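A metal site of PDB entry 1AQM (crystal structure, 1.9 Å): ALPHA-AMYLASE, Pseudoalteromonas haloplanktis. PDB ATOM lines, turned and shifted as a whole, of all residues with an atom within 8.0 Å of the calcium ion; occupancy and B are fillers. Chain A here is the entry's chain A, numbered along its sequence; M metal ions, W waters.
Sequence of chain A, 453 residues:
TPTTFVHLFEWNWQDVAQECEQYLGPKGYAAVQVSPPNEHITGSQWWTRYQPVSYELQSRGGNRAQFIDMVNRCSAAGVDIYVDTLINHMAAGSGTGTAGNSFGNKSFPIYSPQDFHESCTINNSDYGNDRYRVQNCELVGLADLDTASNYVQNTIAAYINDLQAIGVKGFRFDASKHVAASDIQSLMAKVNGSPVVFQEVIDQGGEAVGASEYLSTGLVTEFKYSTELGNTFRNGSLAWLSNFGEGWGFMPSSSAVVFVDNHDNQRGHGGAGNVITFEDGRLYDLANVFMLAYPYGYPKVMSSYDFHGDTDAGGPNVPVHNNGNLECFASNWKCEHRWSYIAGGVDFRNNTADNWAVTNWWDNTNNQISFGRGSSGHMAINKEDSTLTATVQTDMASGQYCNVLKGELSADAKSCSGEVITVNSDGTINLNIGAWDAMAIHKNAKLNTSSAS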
ATOM      1  N   ILE A  87     -23.164  13.885  10.618  1.00  0.00           N
ATOM      2  CA  ILE A  87     -24.313  13.105  11.083  1.00  0.00           C
ATOM      3  C   ILE A  87     -24.823  13.445  12.481  1.00  0.00           C
ATOM      4  O   ILE A  87     -25.870  12.953  12.893  1.00  0.00           O
ATOM      5  CB  ILE A  87     -23.975  11.593  11.069  1.00  0.00           C
ATOM      6  CG1 ILE A  87     -22.800  11.319  12.016  1.00  0.00           C
ATOM      7  CG2 ILE A  87     -23.662  11.134   9.657  1.00  0.00           C
ATOM      8  CD1 ILE A  87     -22.674   9.881  12.447  1.00  0.00           C
ATOM      9  N   ASN A  88     -24.119  14.301  13.200  1.00  0.00           N
ATOM     10  CA  ASN A  88     -24.491  14.633  14.580  1.00  0.00           C
ATOM     11  C   ASN A  88     -25.277  15.918  14.827  1.00  0.00           C
ATOM     12  O   ASN A  88     -26.132  15.960  15.710  1.00  0.00           O
ATOM     13  CB  ASN A  88     -23.226  14.640  15.462  1.00  0.00           C
ATOM     14  CG  ASN A  88     -23.510  15.024  16.922  1.00  0.00           C
ATOM     15  OD1 ASN A  88     -24.084  14.250  17.688  1.00  0.00           O
ATOM     16  ND2 ASN A  88     -23.050  16.211  17.329  1.00  0.00           N
ATOM     17  N   HIS A  89     -25.025  16.951  14.026  1.00  0.00           N
ATOM     18  CA  HIS A  89     -25.643  18.243  14.294  1.00  0.00           C
ATOM     19  C   HIS A  89     -25.907  19.142  13.096  1.00  0.00           C
ATOM     20  O   HIS A  89     -25.582  18.807  11.947  1.00  0.00           O
ATOM     21  CB  HIS A  89     -24.699  18.982  15.244  1.00  0.00           C
ATOM     22  CG  HIS A  89     -23.287  19.085  14.724  1.00  0.00           C
ATOM     23  ND1 HIS A  89     -22.297  18.191  15.087  1.00  0.00           N
ATOM     24  CD2 HIS A  89     -22.723  19.916  13.819  1.00  0.00           C
ATOM     25  CE1 HIS A  89     -21.179  18.478  14.435  1.00  0.00           C
ATOM     26  NE2 HIS A  89     -21.410  19.524  13.656  1.00  0.00           N
ATOM     27  N   HIS A 117     -32.687  16.917  19.851  1.00  0.00           N
ATOM     28  CA  HIS A 117     -32.777  16.585  21.259  1.00  0.00           C
ATOM     29  C   HIS A 117     -32.968  17.906  21.991  1.00  0.00           C
ATOM     30  O   HIS A 117     -32.565  18.959  21.480  1.00  0.00           O
ATOM     31  CB  HIS A 117     -31.463  15.970  21.752  1.00  0.00           C
ATOM     32  CG  HIS A 117     -31.186  14.616  21.204  1.00  0.00           C
ATOM     33  ND1 HIS A 117     -29.928  14.235  20.770  1.00  0.00           N
ATOM     34  CD2 HIS A 117     -31.975  13.527  21.048  1.00  0.00           C
ATOM     35  CE1 HIS A 117     -29.964  12.980  20.391  1.00  0.00           C
ATOM     36  NE2 HIS A 117     -31.187  12.519  20.542  1.00  0.00           N
ATOM     37  N   ILE A 122     -22.724  20.002  26.680  1.00  0.00           N
ATOM     38  CA  ILE A 122     -21.793  18.920  27.001  1.00  0.00           C
ATOM     39  C   ILE A 122     -20.637  19.573  27.772  1.00  0.00           C
ATOM     40  O   ILE A 122     -20.031  20.531  27.291  1.00  0.00           O
ATOM     41  CB  ILE A 122     -21.198  18.239  25.741  1.00  0.00           C
ATOM     42  CG1 ILE A 122     -22.268  17.474  24.963  1.00  0.00           C
ATOM     43  CG2 ILE A 122     -20.065  17.288  26.163  1.00  0.00           C
ATOM     44  CD1 ILE A 122     -21.770  16.841  23.667  1.00  0.00           C
ATOM     45  N   TYR A 132     -24.797   9.645  28.333  1.00  0.00           N
ATOM     46  CA  TYR A 132     -26.072  10.236  27.924  1.00  0.00           C
ATOM     47  C   TYR A 132     -25.876  11.687  27.487  1.00  0.00           C
ATOM     48  O   TYR A 132     -26.382  12.111  26.450  1.00  0.00           O
ATOM     49  CB  TYR A 132     -27.108  10.160  29.048  1.00  0.00           C
ATOM     50  CG  TYR A 132     -28.431  10.784  28.672  1.00  0.00           C
ATOM     51  CD1 TYR A 132     -29.407  10.044  28.001  1.00  0.00           C
ATOM     52  CD2 TYR A 132     -28.678  12.123  28.955  1.00  0.00           C
ATOM     53  CE1 TYR A 132     -30.614  10.644  27.610  1.00  0.00           C
ATOM     54  CE2 TYR A 132     -29.872  12.730  28.577  1.00  0.00           C
ATOM     55  CZ  TYR A 132     -30.842  11.982  27.904  1.00  0.00           C
ATOM     56  OH  TYR A 132     -32.027  12.581  27.538  1.00  0.00           O
ATOM     57  N   ARG A 133     -25.158  12.472  28.301  1.00  0.00           N
ATOM     58  CA  ARG A 133     -24.890  13.871  27.962  1.00  0.00           C
ATOM     59  C   ARG A 133     -23.994  14.027  26.731  1.00  0.00           C
ATOM     60  O   ARG A 133     -24.239  14.884  25.894  1.00  0.00           O
ATOM     61  CB  ARG A 133     -24.319  14.625  29.167  1.00  0.00           C
ATOM     62  CG  ARG A 133     -25.356  14.774  30.297  1.00  0.00           C
ATOM     63  CD  ARG A 133     -24.812  15.591  31.460  1.00  0.00           C
ATOM     64  NE  ARG A 133     -24.580  16.982  31.084  1.00  0.00           N
ATOM     65  CZ  ARG A 133     -25.506  17.929  31.166  1.00  0.00           C
ATOM     66  NH1 ARG A 133     -26.728  17.633  31.584  1.00  0.00           N
ATOM     67  NH2 ARG A 133     -25.207  19.185  30.836  1.00  0.00           N
ATOM     68  N   VAL A 134     -22.954  13.183  26.621  1.00  0.00           N
ATOM     69  CA  VAL A 134     -22.039  13.212  25.465  1.00  0.00           C
ATOM     70  C   VAL A 134     -22.794  13.000  24.136  1.00  0.00           C
ATOM     71  O   VAL A 134     -22.500  13.650  23.126  1.00  0.00           O
ATOM     72  CB  VAL A 134     -20.946  12.097  25.597  1.00  0.00           C
ATOM     73  CG1 VAL A 134     -20.150  11.951  24.295  1.00  0.00           C
ATOM     74  CG2 VAL A 134     -20.004  12.406  26.740  1.00  0.00           C
ATOM     75  N   GLN A 135     -23.802  12.120  24.153  1.00  0.00           N
ATOM     76  CA  GLN A 135     -24.545  11.808  22.938  1.00  0.00           C
ATOM     77  C   GLN A 135     -25.869  12.511  22.739  1.00  0.00           C
ATOM     78  O   GLN A 135     -26.401  12.514  21.626  1.00  0.00           O
ATOM     79  CB  GLN A 135     -24.717  10.288  22.828  1.00  0.00           C
ATOM     80  CG  GLN A 135     -23.373   9.559  22.842  1.00  0.00           C
ATOM     81  CD  GLN A 135     -23.493   8.053  22.666  1.00  0.00           C
ATOM     82  OE1 GLN A 135     -24.532   7.450  22.963  1.00  0.00           O
ATOM     83  NE2 GLN A 135     -22.419   7.433  22.166  1.00  0.00           N
ATOM     84  N   ASN A 136     -26.407  13.138  23.777  1.00  0.00           N
ATOM     85  CA  ASN A 136     -27.686  13.815  23.626  1.00  0.00           C
ATOM     86  C   ASN A 136     -27.633  15.325  23.793  1.00  0.00           C
ATOM     87  O   ASN A 136     -28.538  16.028  23.375  1.00  0.00           O
ATOM     88  CB  ASN A 136     -28.744  13.183  24.543  1.00  0.00           C
ATOM     89  CG  ASN A 136     -29.100  11.775  24.113  1.00  0.00           C
ATOM     90  OD1 ASN A 136     -29.940  11.579  23.238  1.00  0.00           O
ATOM     91  ND2 ASN A 136     -28.442  10.792  24.703  1.00  0.00           N
ATOM     92  N   CYS A 137     -26.546  15.817  24.402  1.00  0.00           N
ATOM     93  CA  CYS A 137     -26.394  17.259  24.583  1.00  0.00           C
ATOM     94  C   CYS A 137     -25.615  17.895  23.421  1.00  0.00           C
ATOM     95  O   CYS A 137     -25.078  17.184  22.552  1.00  0.00           O
ATOM     96  CB  CYS A 137     -25.761  17.588  25.941  1.00  0.00           C
ATOM     97  SG  CYS A 137     -26.845  17.099  27.331  1.00  0.00           S
ATOM     98  N   GLU A 138     -25.510  19.218  23.439  1.00  0.00           N
ATOM     99  CA  GLU A 138     -24.852  19.959  22.376  1.00  0.00           C
ATOM    100  C   GLU A 138     -23.336  20.127  22.458  1.00  0.00           C
ATOM    101  O   GLU A 138     -22.787  20.451  23.507  1.00  0.00           O
ATOM    102  CB  GLU A 138     -25.498  21.325  22.207  1.00  0.00           C
ATOM    103  CG  GLU A 138     -26.982  21.237  21.892  1.00  0.00           C
ATOM    104  CD  GLU A 138     -27.714  22.566  21.988  1.00  0.00           C
ATOM    105  OE1 GLU A 138     -27.193  23.522  22.588  1.00  0.00           O
ATOM    106  OE2 GLU A 138     -28.856  22.635  21.456  1.00  0.00           O
ATOM    107  N   LEU A 139     -22.681  19.857  21.326  1.00  0.00           N
ATOM    108  CA  LEU A 139     -21.247  20.020  21.179  1.00  0.00           C
ATOM    109  C   LEU A 139     -21.043  21.499  20.828  1.00  0.00           C
ATOM    110  O   LEU A 139     -21.456  21.949  19.754  1.00  0.00           O
ATOM    111  CB  LEU A 139     -20.741  19.137  20.033  1.00  0.00           C
ATOM    112  CG  LEU A 139     -19.264  19.226  19.643  1.00  0.00           C
ATOM    113  CD1 LEU A 139     -18.382  18.888  20.841  1.00  0.00           C
ATOM    114  CD2 LEU A 139     -18.993  18.260  18.484  1.00  0.00           C
ATOM    115  N   LEU A 142     -23.852  23.481  19.015  1.00  0.00           N
ATOM    116  CA  LEU A 142     -24.422  22.963  17.773  1.00  0.00           C
ATOM    117  C   LEU A 142     -25.712  22.166  18.032  1.00  0.00           C
ATOM    118  O   LEU A 142     -25.750  21.326  18.928  1.00  0.00           O
ATOM    119  CB  LEU A 142     -23.380  22.098  17.042  1.00  0.00           C
ATOM    120  CG  LEU A 142     -22.077  22.842  16.706  1.00  0.00           C
ATOM    121  CD1 LEU A 142     -21.013  21.874  16.210  1.00  0.00           C
ATOM    122  CD2 LEU A 142     -22.360  23.935  15.679  1.00  0.00           C
ATOM    123  N   ALA A 143     -26.767  22.481  17.282  1.00  0.00           N
ATOM    124  CA  ALA A 143     -28.066  21.808  17.456  1.00  0.00           C
ATOM    125  C   ALA A 143     -27.921  20.297  17.282  1.00  0.00           C
ATOM    126  O   ALA A 143     -27.539  19.810  16.216  1.00  0.00           O
ATOM    127  CB  ALA A 143     -29.078  22.375  16.467  1.00  0.00           C
ATOM    128  N   ASP A 144     -28.189  19.554  18.355  1.00  0.00           N
ATOM    129  CA  ASP A 144     -28.036  18.107  18.341  1.00  0.00           C
ATOM    130  C   ASP A 144     -29.228  17.344  17.743  1.00  0.00           C
ATOM    131  O   ASP A 144     -30.287  17.275  18.339  1.00  0.00           O
ATOM    132  CB  ASP A 144     -27.743  17.604  19.758  1.00  0.00           C
ATOM    133  CG  ASP A 144     -26.929  16.305  19.763  1.00  0.00           C
ATOM    134  OD1 ASP A 144     -25.759  16.328  19.318  1.00  0.00           O
ATOM    135  OD2 ASP A 144     -27.450  15.278  20.211  1.00  0.00           O
ATOM    136  N   LEU A 145     -29.026  16.733  16.566  1.00  0.00           N
ATOM    137  CA  LEU A 145     -30.075  15.992  15.879  1.00  0.00           C
ATOM    138  C   LEU A 145     -30.551  14.751  16.637  1.00  0.00           C
ATOM    139  O   LEU A 145     -29.758  14.077  17.321  1.00  0.00           O
ATOM    140  CB  LEU A 145     -29.608  15.532  14.475  1.00  0.00           C
ATOM    141  CG  LEU A 145     -29.480  16.519  13.290  1.00  0.00           C
ATOM    142  CD1 LEU A 145     -28.660  15.906  12.160  1.00  0.00           C
ATOM    143  CD2 LEU A 145     -30.850  16.879  12.793  1.00  0.00           C
ATOM    144  N   ASP A 146     -31.835  14.455  16.541  1.00  0.00           N
ATOM    145  CA  ASP A 146     -32.366  13.249  17.160  1.00  0.00           C
ATOM    146  C   ASP A 146     -32.089  12.106  16.156  1.00  0.00           C
ATOM    147  O   ASP A 146     -32.939  11.738  15.353  1.00  0.00           O
ATOM    148  CB  ASP A 146     -33.862  13.390  17.458  1.00  0.00           C
ATOM    149  CG  ASP A 146     -34.462  12.152  18.109  1.00  0.00           C
ATOM    150  OD1 ASP A 146     -33.735  11.148  18.348  1.00  0.00           O
ATOM    151  OD2 ASP A 146     -35.678  12.193  18.372  1.00  0.00           O
ATOM    152  N   THR A 147     -30.879  11.554  16.240  1.00  0.00           N
ATOM    153  CA  THR A 147     -30.441  10.499  15.341  1.00  0.00           C
ATOM    154  C   THR A 147     -31.193   9.163  15.510  1.00  0.00           C
ATOM    155  O   THR A 147     -30.934   8.207  14.778  1.00  0.00           O
ATOM    156  CB  THR A 147     -28.900  10.320  15.422  1.00  0.00           C
ATOM    157  OG1 THR A 147     -28.499  10.147  16.786  1.00  0.00           O
ATOM    158  CG2 THR A 147     -28.209  11.554  14.883  1.00  0.00           C
ATOM    159  N   ALA A 175     -17.898  13.623  14.084  1.00  0.00           N
ATOM    160  CA  ALA A 175     -18.423  13.616  15.458  1.00  0.00           C
ATOM    161  C   ALA A 175     -19.203  12.338  15.816  1.00  0.00           C
ATOM    162  O   ALA A 175     -20.231  12.404  16.486  1.00  0.00           O
ATOM    163  CB  ALA A 175     -19.300  14.863  15.684  1.00  0.00           C
ATOM    164  N   SER A 176     -18.694  11.183  15.388  1.00  0.00           N
ATOM    165  CA  SER A 176     -19.345   9.893  15.642  1.00  0.00           C
ATOM    166  C   SER A 176     -19.523   9.559  17.116  1.00  0.00           C
ATOM    167  O   SER A 176     -20.507   8.908  17.480  1.00  0.00           O
ATOM    168  CB  SER A 176     -18.597   8.765  14.950  1.00  0.00           C
ATOM    169  OG  SER A 176     -18.772   8.836  13.546  1.00  0.00           O
ATOM    170  N   LYS A 177     -18.582   9.977  17.949  1.00  0.00           N
ATOM    171  CA  LYS A 177     -18.673   9.712  19.397  1.00  0.00           C
ATOM    172  C   LYS A 177     -19.935  10.331  20.024  1.00  0.00           C
ATOM    173  O   LYS A 177     -20.473   9.807  21.012  1.00  0.00           O
ATOM    174  CB  LYS A 177     -17.415  10.224  20.113  1.00  0.00           C
ATOM    175  CG  LYS A 177     -17.392   9.898  21.602  1.00  0.00           C
ATOM    176  CD  LYS A 177     -15.990  10.013  22.184  1.00  0.00           C
ATOM    177  CE  LYS A 177     -15.621  11.440  22.427  1.00  0.00           C
ATOM    178  NZ  LYS A 177     -14.200  11.524  22.846  1.00  0.00           N
ATOM    179  N   HIS A 178     -20.436  11.397  19.417  1.00  0.00           N
ATOM    180  CA  HIS A 178     -21.612  12.091  19.917  1.00  0.00           C
ATOM    181  C   HIS A 178     -22.919  11.486  19.428  1.00  0.00           C
ATOM    182  O   HIS A 178     -24.000  12.017  19.701  1.00  0.00           O
ATOM    183  CB  HIS A 178     -21.497  13.580  19.626  1.00  0.00           C
ATOM    184  CG  HIS A 178     -20.267  14.209  20.217  1.00  0.00           C
ATOM    185  ND1 HIS A 178     -20.204  14.640  21.524  1.00  0.00           N
ATOM    186  CD2 HIS A 178     -19.021  14.401  19.709  1.00  0.00           C
ATOM    187  CE1 HIS A 178     -18.982  15.071  21.796  1.00  0.00           C
ATOM    188  NE2 HIS A 178     -18.247  14.939  20.715  1.00  0.00           N
ATOM    189  N   VAL A 179     -22.823  10.352  18.730  1.00  0.00           N
ATOM    190  CA  VAL A 179     -24.000   9.646  18.226  1.00  0.00           C
ATOM    191  C   VAL A 179     -23.891   8.201  18.695  1.00  0.00           C
ATOM    192  O   VAL A 179     -22.837   7.577  18.544  1.00  0.00           O
ATOM    193  CB  VAL A 179     -24.089   9.659  16.667  1.00  0.00           C
ATOM    194  CG1 VAL A 179     -25.280   8.836  16.188  1.00  0.00           C
ATOM    195  CG2 VAL A 179     -24.156  11.085  16.131  1.00  0.00           C
ATOM    196  N   ALA A 180     -24.968   7.678  19.291  1.00  0.00           N
ATOM    197  CA  ALA A 180     -24.960   6.283  19.760  1.00  0.00           C
ATOM    198  C   ALA A 180     -24.609   5.322  18.623  1.00  0.00           C
ATOM    199  O   ALA A 180     -25.118   5.457  17.499  1.00  0.00           O
ATOM    200  CB  ALA A 180     -26.322   5.922  20.373  1.00  0.00           C
ATOM    201  N   ASP A 183     -27.501   4.036  16.754  1.00  0.00           N
ATOM    202  CA  ASP A 183     -28.143   4.970  15.820  1.00  0.00           C
ATOM    203  C   ASP A 183     -27.422   4.878  14.470  1.00  0.00           C
ATOM    204  O   ASP A 183     -28.058   5.005  13.425  1.00  0.00           O
ATOM    205  CB  ASP A 183     -28.078   6.422  16.334  1.00  0.00           C
ATOM    206  CG  ASP A 183     -29.071   6.696  17.448  1.00  0.00           C
ATOM    207  OD1 ASP A 183     -29.870   5.805  17.808  1.00  0.00           O
ATOM    208  OD2 ASP A 183     -29.054   7.818  17.981  1.00  0.00           O
HETATM  209 CA    CA M   1     -25.696  13.722  19.408  1.00  0.00          CA
HETATM  210  O   HOH W   1     -26.954  13.904  17.413  1.00  0.00           O
HETATM  211  O   HOH W   2     -27.141  11.690  18.922  1.00  0.00           O
HETATM  212  O   HOH W   3     -24.223  14.870  21.279  1.00  0.00           O
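The backbone carbonyl oxygen of Asn 88 lies within hydrogen-bond range of the backbone NH of Leu 145 (3.1 Å).
The side-chain amide nitrogen (ND2) of Asn 88 is in hydrogen-bond range of a ring nitrogen (ND1) of His 89 (3.1 Å).
O of Val 134 sits at hydrogen-bond distance from ND1 of His 178, 3.0 Å away.
N of His 117 is in hydrogen-bond range of O of Asp 144.
O of Lys 177 sits at hydrogen-bond distance from NE2 of Gln 135, 3.3 Å away.
The calcium ion is bound by water W1, 2.4 Å away.
OD1 of Asn 88 is bound to the calcium ion.
O of His 178 binds the calcium ion.
The calcium ion is bound by the side-chain carboxylate (OD2) of Asp 144, at 2.5 Å.
The calcium ion is bound by water W2 (2.5 Å).
OD1 of Asp 144 is bound to the calcium ion (2.6 Å).
O of Gln 135 binds the calcium ion.
Water W3 binds the calcium ion (2.6 Å).
The calcium ion has eight donor atoms within binding distance.
Water W1 bridges O of Asn 88 (2.8 Å) and O of Leu 145 (2.8 Å).
Within 4 Å of the calcium ion: Asn 88, Gln 135, Asp 144 and His 178.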
